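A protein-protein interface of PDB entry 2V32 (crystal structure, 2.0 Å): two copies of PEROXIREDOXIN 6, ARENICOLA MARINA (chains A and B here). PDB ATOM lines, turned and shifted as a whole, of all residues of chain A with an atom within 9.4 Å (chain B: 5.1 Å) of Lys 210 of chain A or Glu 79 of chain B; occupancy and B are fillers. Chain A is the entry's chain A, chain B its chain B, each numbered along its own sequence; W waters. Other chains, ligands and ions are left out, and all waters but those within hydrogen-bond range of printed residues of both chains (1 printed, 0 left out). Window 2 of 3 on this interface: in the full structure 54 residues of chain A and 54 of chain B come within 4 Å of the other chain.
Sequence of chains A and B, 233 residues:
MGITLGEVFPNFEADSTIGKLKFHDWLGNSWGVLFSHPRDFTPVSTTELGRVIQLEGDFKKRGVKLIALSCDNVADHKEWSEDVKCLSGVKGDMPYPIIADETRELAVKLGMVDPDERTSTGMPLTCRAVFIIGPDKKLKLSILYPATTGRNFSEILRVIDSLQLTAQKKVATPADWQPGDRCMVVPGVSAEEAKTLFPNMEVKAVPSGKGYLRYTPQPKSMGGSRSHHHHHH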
ATOM      1  N   VAL A 203     -29.596 -14.338   4.217  1.00  0.00           N
ATOM      2  CA  VAL A 203     -29.204 -15.094   5.408  1.00  0.00           C
ATOM      3  C   VAL A 203     -28.556 -16.390   4.907  1.00  0.00           C
ATOM      4  O   VAL A 203     -29.233 -17.230   4.297  1.00  0.00           O
ATOM      5  CB  VAL A 203     -30.400 -15.348   6.384  1.00  0.00           C
ATOM      6  CG1 VAL A 203     -29.988 -16.182   7.611  1.00  0.00           C
ATOM      7  CG2 VAL A 203     -31.101 -13.995   6.809  1.00  0.00           C
ATOM      8  N   LYS A 204     -27.250 -16.547   5.147  1.00  0.00           N
ATOM      9  CA  LYS A 204     -26.499 -17.759   4.769  1.00  0.00           C
ATOM     10  C   LYS A 204     -26.625 -18.801   5.878  1.00  0.00           C
ATOM     11  O   LYS A 204     -26.306 -18.553   7.025  1.00  0.00           O
ATOM     12  CB  LYS A 204     -25.033 -17.453   4.529  1.00  0.00           C
ATOM     13  CG  LYS A 204     -24.162 -18.685   4.066  1.00  0.00           C
ATOM     14  CD  LYS A 204     -22.662 -18.323   3.888  1.00  0.00           C
ATOM     15  CE  LYS A 204     -21.942 -19.169   2.766  1.00  0.00           C
ATOM     16  NZ  LYS A 204     -22.381 -20.596   2.730  1.00  0.00           N
ATOM     17  N   ALA A 205     -27.134 -19.961   5.527  1.00  0.00           N
ATOM     18  CA  ALA A 205     -27.296 -21.022   6.495  1.00  0.00           C
ATOM     19  C   ALA A 205     -25.889 -21.454   6.932  1.00  0.00           C
ATOM     20  O   ALA A 205     -24.959 -21.442   6.147  1.00  0.00           O
ATOM     21  CB  ALA A 205     -28.052 -22.164   5.878  1.00  0.00           C
ATOM     22  N   VAL A 206     -25.749 -21.782   8.194  1.00  0.00           N
ATOM     23  CA  VAL A 206     -24.471 -22.178   8.784  1.00  0.00           C
ATOM     24  C   VAL A 206     -24.764 -23.441   9.632  1.00  0.00           C
ATOM     25  O   VAL A 206     -25.930 -23.651   9.999  1.00  0.00           O
ATOM     26  CB  VAL A 206     -23.866 -21.003   9.581  1.00  0.00           C
ATOM     27  CG1 VAL A 206     -23.159 -19.987   8.616  1.00  0.00           C
ATOM     28  CG2 VAL A 206     -24.916 -20.247  10.371  1.00  0.00           C
ATOM     29  N   PRO A 207     -23.752 -24.322   9.867  1.00  0.00           N
ATOM     30  CA  PRO A 207     -24.050 -25.533  10.630  1.00  0.00           C
ATOM     31  C   PRO A 207     -24.762 -25.319  11.979  1.00  0.00           C
ATOM     32  O   PRO A 207     -25.520 -26.174  12.385  1.00  0.00           O
ATOM     33  CB  PRO A 207     -22.679 -26.238  10.808  1.00  0.00           C
ATOM     34  CG  PRO A 207     -21.756 -25.666   9.833  1.00  0.00           C
ATOM     35  CD  PRO A 207     -22.347 -24.257   9.433  1.00  0.00           C
ATOM     36  N   SER A 208     -24.521 -24.191  12.659  1.00  0.00           N
ATOM     37  CA  SER A 208     -25.142 -23.942  13.954  1.00  0.00           C
ATOM     38  C   SER A 208     -26.641 -23.755  13.877  1.00  0.00           C
ATOM     39  O   SER A 208     -27.314 -23.819  14.916  1.00  0.00           O
ATOM     40  CB  SER A 208     -24.517 -22.725  14.651  1.00  0.00           C
ATOM     41  OG  SER A 208     -24.967 -21.513  14.096  1.00  0.00           O
ATOM     42  N   GLY A 209     -27.160 -23.488  12.663  1.00  0.00           N
ATOM     43  CA  GLY A 209     -28.599 -23.231  12.480  1.00  0.00           C
ATOM     44  C   GLY A 209     -28.963 -21.832  12.910  1.00  0.00           C
ATOM     45  O   GLY A 209     -30.136 -21.444  12.859  1.00  0.00           O
ATOM     46  N   LYS A 210     -27.991 -21.067  13.387  1.00  0.00           N
ATOM     47  CA  LYS A 210     -28.300 -19.674  13.760  1.00  0.00           C
ATOM     48  C   LYS A 210     -28.434 -18.769  12.495  1.00  0.00           C
ATOM     49  O   LYS A 210     -27.902 -19.109  11.409  1.00  0.00           O
ATOM     50  CB  LYS A 210     -27.305 -19.122  14.789  1.00  0.00           C
ATOM     51  CG  LYS A 210     -26.891 -20.151  15.843  1.00  0.00           C
ATOM     52  CD  LYS A 210     -26.164 -19.553  16.978  1.00  0.00           C
ATOM     53  CE  LYS A 210     -25.768 -20.644  17.963  1.00  0.00           C
ATOM     54  NZ  LYS A 210     -26.687 -20.525  19.109  1.00  0.00           N
ATOM     55  N   GLY A 211     -29.093 -17.616  12.656  1.00  0.00           N
ATOM     56  CA  GLY A 211     -29.481 -16.774  11.512  1.00  0.00           C
ATOM     57  C   GLY A 211     -28.718 -15.469  11.457  1.00  0.00           C
ATOM     58  O   GLY A 211     -29.224 -14.477  10.957  1.00  0.00           O
ATOM     59  N   TYR A 212     -27.467 -15.500  11.923  1.00  0.00           N
ATOM     60  CA  TYR A 212     -26.674 -14.287  12.124  1.00  0.00           C
ATOM     61  C   TYR A 212     -25.781 -13.970  10.919  1.00  0.00           C
ATOM     62  O   TYR A 212     -25.213 -12.902  10.858  1.00  0.00           O
ATOM     63  CB  TYR A 212     -25.763 -14.416  13.355  1.00  0.00           C
ATOM     64  CG  TYR A 212     -24.648 -15.447  13.135  1.00  0.00           C
ATOM     65  CD1 TYR A 212     -23.466 -15.116  12.473  1.00  0.00           C
ATOM     66  CD2 TYR A 212     -24.794 -16.768  13.573  1.00  0.00           C
ATOM     67  CE1 TYR A 212     -22.481 -16.045  12.285  1.00  0.00           C
ATOM     68  CE2 TYR A 212     -23.801 -17.725  13.336  1.00  0.00           C
ATOM     69  CZ  TYR A 212     -22.665 -17.359  12.690  1.00  0.00           C
ATOM     70  OH  TYR A 212     -21.647 -18.312  12.484  1.00  0.00           O
ATOM     71  N   LEU A 213     -25.580 -14.912  10.016  1.00  0.00           N
ATOM     72  CA  LEU A 213     -24.644 -14.643   8.925  1.00  0.00           C
ATOM     73  C   LEU A 213     -25.391 -13.879   7.837  1.00  0.00           C
ATOM     74  O   LEU A 213     -25.812 -14.486   6.866  1.00  0.00           O
ATOM     75  CB  LEU A 213     -24.072 -15.930   8.374  1.00  0.00           C
ATOM     76  CG  LEU A 213     -22.726 -15.795   7.641  1.00  0.00           C
ATOM     77  CD1 LEU A 213     -21.655 -15.236   8.596  1.00  0.00           C
ATOM     78  CD2 LEU A 213     -22.250 -17.177   7.129  1.00  0.00           C
ATOM     79  N   ARG A 214     -25.544 -12.559   7.989  1.00  0.00           N
ATOM     80  CA  ARG A 214     -26.438 -11.806   7.098  1.00  0.00           C
ATOM     81  C   ARG A 214     -25.680 -10.724   6.284  1.00  0.00           C
ATOM     82  O   ARG A 214     -24.997  -9.918   6.873  1.00  0.00           O
ATOM     83  CB  ARG A 214     -27.579 -11.168   7.915  1.00  0.00           C
ATOM     84  CG  ARG A 214     -28.365 -12.202   8.767  1.00  0.00           C
ATOM     85  CD  ARG A 214     -29.542 -11.595   9.519  1.00  0.00           C
ATOM     86  NE  ARG A 214     -29.171 -10.697  10.609  1.00  0.00           N
ATOM     87  CZ  ARG A 214     -30.023  -9.898  11.237  1.00  0.00           C
ATOM     88  NH1 ARG A 214     -31.321  -9.913  10.947  1.00  0.00           N
ATOM     89  NH2 ARG A 214     -29.598  -9.110  12.196  1.00  0.00           N
ATOM     90  N   PHE B  41     -20.538 -16.250  16.927  1.00  0.00           N
ATOM     91  CA  PHE B  41     -21.866 -16.263  16.247  1.00  0.00           C
ATOM     92  C   PHE B  41     -22.236 -14.868  15.825  1.00  0.00           C
ATOM     93  O   PHE B  41     -23.360 -14.445  16.004  1.00  0.00           O
ATOM     94  CB  PHE B  41     -22.968 -16.865  17.131  1.00  0.00           C
ATOM     95  CG  PHE B  41     -22.651 -18.291  17.654  1.00  0.00           C
ATOM     96  CD1 PHE B  41     -22.567 -19.364  16.799  1.00  0.00           C
ATOM     97  CD2 PHE B  41     -22.490 -18.525  19.023  1.00  0.00           C
ATOM     98  CE1 PHE B  41     -22.317 -20.654  17.286  1.00  0.00           C
ATOM     99  CE2 PHE B  41     -22.214 -19.789  19.507  1.00  0.00           C
ATOM    100  CZ  PHE B  41     -22.143 -20.844  18.648  1.00  0.00           C
ATOM    101  N   ALA B  75     -17.143 -23.870  25.200  1.00  0.00           N
ATOM    102  CA  ALA B  75     -18.232 -24.554  24.495  1.00  0.00           C
ATOM    103  C   ALA B  75     -18.760 -23.745  23.289  1.00  0.00           C
ATOM    104  O   ALA B  75     -18.984 -24.274  22.233  1.00  0.00           O
ATOM    105  CB  ALA B  75     -19.373 -24.889  25.458  1.00  0.00           C
ATOM    106  N   ASP B  76     -18.967 -22.456  23.465  1.00  0.00           N
ATOM    107  CA  ASP B  76     -19.423 -21.601  22.336  1.00  0.00           C
ATOM    108  C   ASP B  76     -18.383 -21.514  21.233  1.00  0.00           C
ATOM    109  O   ASP B  76     -18.699 -21.660  20.070  1.00  0.00           O
ATOM    110  CB  ASP B  76     -19.798 -20.212  22.844  1.00  0.00           C
ATOM    111  CG  ASP B  76     -21.177 -20.174  23.449  1.00  0.00           C
ATOM    112  OD1 ASP B  76     -21.827 -21.232  23.571  1.00  0.00           O
ATOM    113  OD2 ASP B  76     -21.622 -19.053  23.815  1.00  0.00           O
ATOM    114  N   HIS B  77     -17.137 -21.314  21.633  1.00  0.00           N
ATOM    115  CA  HIS B  77     -16.001 -21.420  20.700  1.00  0.00           C
ATOM    116  C   HIS B  77     -16.073 -22.676  19.808  1.00  0.00           C
ATOM    117  O   HIS B  77     -16.044 -22.564  18.598  1.00  0.00           O
ATOM    118  CB  HIS B  77     -14.646 -21.290  21.445  1.00  0.00           C
ATOM    119  CG  HIS B  77     -14.399 -19.918  22.039  1.00  0.00           C
ATOM    120  ND1 HIS B  77     -13.325 -19.640  22.858  1.00  0.00           N
ATOM    121  CD2 HIS B  77     -15.095 -18.761  21.943  1.00  0.00           C
ATOM    122  CE1 HIS B  77     -13.355 -18.371  23.229  1.00  0.00           C
ATOM    123  NE2 HIS B  77     -14.436 -17.822  22.700  1.00  0.00           N
ATOM    124  N   LYS B  78     -16.142 -23.864  20.417  1.00  0.00           N
ATOM    125  CA  LYS B  78     -16.147 -25.106  19.664  1.00  0.00           C
ATOM    126  C   LYS B  78     -17.313 -25.194  18.693  1.00  0.00           C
ATOM    127  O   LYS B  78     -17.136 -25.588  17.542  1.00  0.00           O
ATOM    128  CB  LYS B  78     -16.165 -26.292  20.621  1.00  0.00           C
ATOM    129  CG  LYS B  78     -14.794 -26.486  21.141  1.00  0.00           C
ATOM    130  CD  LYS B  78     -14.765 -27.115  22.492  1.00  0.00           C
ATOM    131  CE  LYS B  78     -13.302 -27.430  22.881  1.00  0.00           C
ATOM    132  NZ  LYS B  78     -13.359 -28.451  23.987  1.00  0.00           N
ATOM    133  N   GLU B  79     -18.503 -24.822  19.153  1.00  0.00           N
ATOM    134  CA  GLU B  79     -19.677 -24.851  18.283  1.00  0.00           C
ATOM    135  C   GLU B  79     -19.566 -23.780  17.187  1.00  0.00           C
ATOM    136  O   GLU B  79     -19.798 -24.077  16.053  1.00  0.00           O
ATOM    137  CB  GLU B  79     -20.952 -24.682  19.096  1.00  0.00           C
ATOM    138  CG  GLU B  79     -22.235 -24.915  18.298  1.00  0.00           C
ATOM    139  CD  GLU B  79     -23.483 -24.413  18.991  1.00  0.00           C
ATOM    140  OE1 GLU B  79     -23.423 -24.047  20.210  1.00  0.00           O
ATOM    141  OE2 GLU B  79     -24.515 -24.354  18.277  1.00  0.00           O
ATOM    142  N   TRP B  80     -19.170 -22.555  17.517  1.00  0.00           N
ATOM    143  CA  TRP B  80     -19.064 -21.496  16.483  1.00  0.00           C
ATOM    144  C   TRP B  80     -17.970 -21.780  15.465  1.00  0.00           C
ATOM    145  O   TRP B  80     -18.071 -21.380  14.321  1.00  0.00           O
ATOM    146  CB  TRP B  80     -18.801 -20.151  17.137  1.00  0.00           C
ATOM    147  CG  TRP B  80     -18.625 -19.059  16.166  1.00  0.00           C
ATOM    148  CD1 TRP B  80     -19.445 -18.744  15.122  1.00  0.00           C
ATOM    149  CD2 TRP B  80     -17.586 -18.109  16.163  1.00  0.00           C
ATOM    150  NE1 TRP B  80     -18.958 -17.670  14.449  1.00  0.00           N
ATOM    151  CE2 TRP B  80     -17.827 -17.240  15.075  1.00  0.00           C
ATOM    152  CE3 TRP B  80     -16.443 -17.920  16.951  1.00  0.00           C
ATOM    153  CZ2 TRP B  80     -16.983 -16.194  14.766  1.00  0.00           C
ATOM    154  CZ3 TRP B  80     -15.622 -16.870  16.662  1.00  0.00           C
ATOM    155  CH2 TRP B  80     -15.890 -16.015  15.573  1.00  0.00           C
ATOM    156  N   SER B  81     -16.934 -22.483  15.899  1.00  0.00           N
ATOM    157  CA  SER B  81     -15.833 -22.917  15.045  1.00  0.00           C
ATOM    158  C   SER B  81     -16.277 -23.757  13.837  1.00  0.00           C
ATOM    159  O   SER B  81     -15.678 -23.672  12.761  1.00  0.00           O
ATOM    160  CB  SER B  81     -14.812 -23.695  15.861  1.00  0.00           C
ATOM    161  OG  SER B  81     -14.025 -22.830  16.669  1.00  0.00           O
ATOM    162  N   GLU B  82     -17.316 -24.568  14.007  1.00  0.00           N
ATOM    163  CA  GLU B  82     -17.918 -25.262  12.864  1.00  0.00           C
ATOM    164  C   GLU B  82     -18.470 -24.319  11.761  1.00  0.00           C
ATOM    165  O   GLU B  82     -18.234 -24.556  10.584  1.00  0.00           O
ATOM    166  CB  GLU B  82     -18.916 -26.321  13.355  1.00  0.00           C
ATOM    167  CG  GLU B  82     -18.265 -27.455  14.211  1.00  0.00           C
ATOM    168  CD  GLU B  82     -16.979 -28.129  13.593  1.00  0.00           C
ATOM    169  OE1 GLU B  82     -16.984 -28.581  12.420  1.00  0.00           O
ATOM    170  OE2 GLU B  82     -15.954 -28.254  14.294  1.00  0.00           O
ATOM    171  N   ASP B  83     -19.149 -23.234  12.140  1.00  0.00           N
ATOM    172  CA  ASP B  83     -19.526 -22.169  11.170  1.00  0.00           C
ATOM    173  C   ASP B  83     -18.340 -21.446  10.483  1.00  0.00           C
ATOM    174  O   ASP B  83     -18.389 -21.109   9.257  1.00  0.00           O
ATOM    175  CB  ASP B  83     -20.393 -21.066  11.845  1.00  0.00           C
ATOM    176  CG  ASP B  83     -21.614 -21.597  12.568  1.00  0.00           C
ATOM    177  OD1 ASP B  83     -21.832 -22.838  12.581  1.00  0.00           O
ATOM    178  OD2 ASP B  83     -22.366 -20.749  13.125  1.00  0.00           O
HETATM  179  O   HOH W   1     -21.780 -24.702  14.432  1.00  0.00           O
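Of the 12 printed residues of chain A, 5 touch a printed residue of chain B. Along chain A the printed residues that touch a printed residue of chain B span positions 206 to 212. Printed residues of chain B that touch a printed residue of chain A: Phe 41, Glu 79, Trp 80, Glu 82 and Asp 83. Among the printed residues, no Asp or Glu carboxylate lies within 4 Å of a Lys or Arg side-chain nitrogen of the other chain.
OG of Ser 208 of chain A lies within hydrogen-bond range of OD2 of Asp 83 of chain B (2.9 Å). OH of Tyr 212 of chain A sits at hydrogen-bond distance from NE1 of Trp 80 of chain B (3.4 Å). OH of Tyr 212 of chain A lies within hydrogen-bond range of OD2 of Asp 83 of chain B, at 2.6 Å.
No position is printed for both chains.
Water W1 lies within hydrogen-bond range of the side-chain carboxylate (OD1) of Asp 83 of chain B (2.6 Å), the backbone carbonyl oxygen (O) of Glu 79 of chain B (2.6 Å) and the backbone NH (N) of Ser 208 of chain A (3.3 Å).
The side-chain hydroxyl (OG) of Ser 208 of chain A lies close to the backbone NH (N) of Lys 210 of chain A, at 3.1 Å.
Val 206 of chain A touches Asp 83 of chain B. Pro 207 of chain A touches Glu 82 of chain B (CG to O, 3.8 Å). Asp 83 of chain B touches Pro 207 of chain A (OD1 to CD, 3.5 Å). Glu 79 of chain B touches Ser 208 of chain A. Phe 41 of chain B touches Lys 210 of chain A (CE1 to CE, 3.5 Å). CE of Lys 210 of chain A touches OE2 of Glu 79 of chain B (3.9 Å). Tyr 212 of chain A touches Phe 41 of chain B.
Of the printed residues of chain B, Val 206 of chain A touches Asp 83. Lys 210 of chain A touches two residues of chain B. Of the printed residues of chain B, Tyr 212 of chain A touches Phe 41 (3.3 Å), Trp 80 (3.4 Å) and Asp 83 (2.6 Å). Of chain A, only Ser 208 (3.98 Å) and Lys 210 (3.9 Å) come within 4 Å of Glu 79 of chain B. Printed residues of chain A within 4 Å of Asp 83 of chain B: Val 206 (3.8 Å), Pro 207 (3.5 Å), Ser 208 (2.9 Å) and Tyr 212 (2.6 Å). The nearest printed residue of chain B that does not touch Lys 210 of chain A is Asp 83 of chain B (5.3 Å). The nearest printed residue of chain A that does not touch Glu 79 of chain B is Pro 207 of chain A (6.2 Å). The nearest printed residue of chain A that does not touch Asp 83 of chain B is Lys 210 of chain A (5.3 Å).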
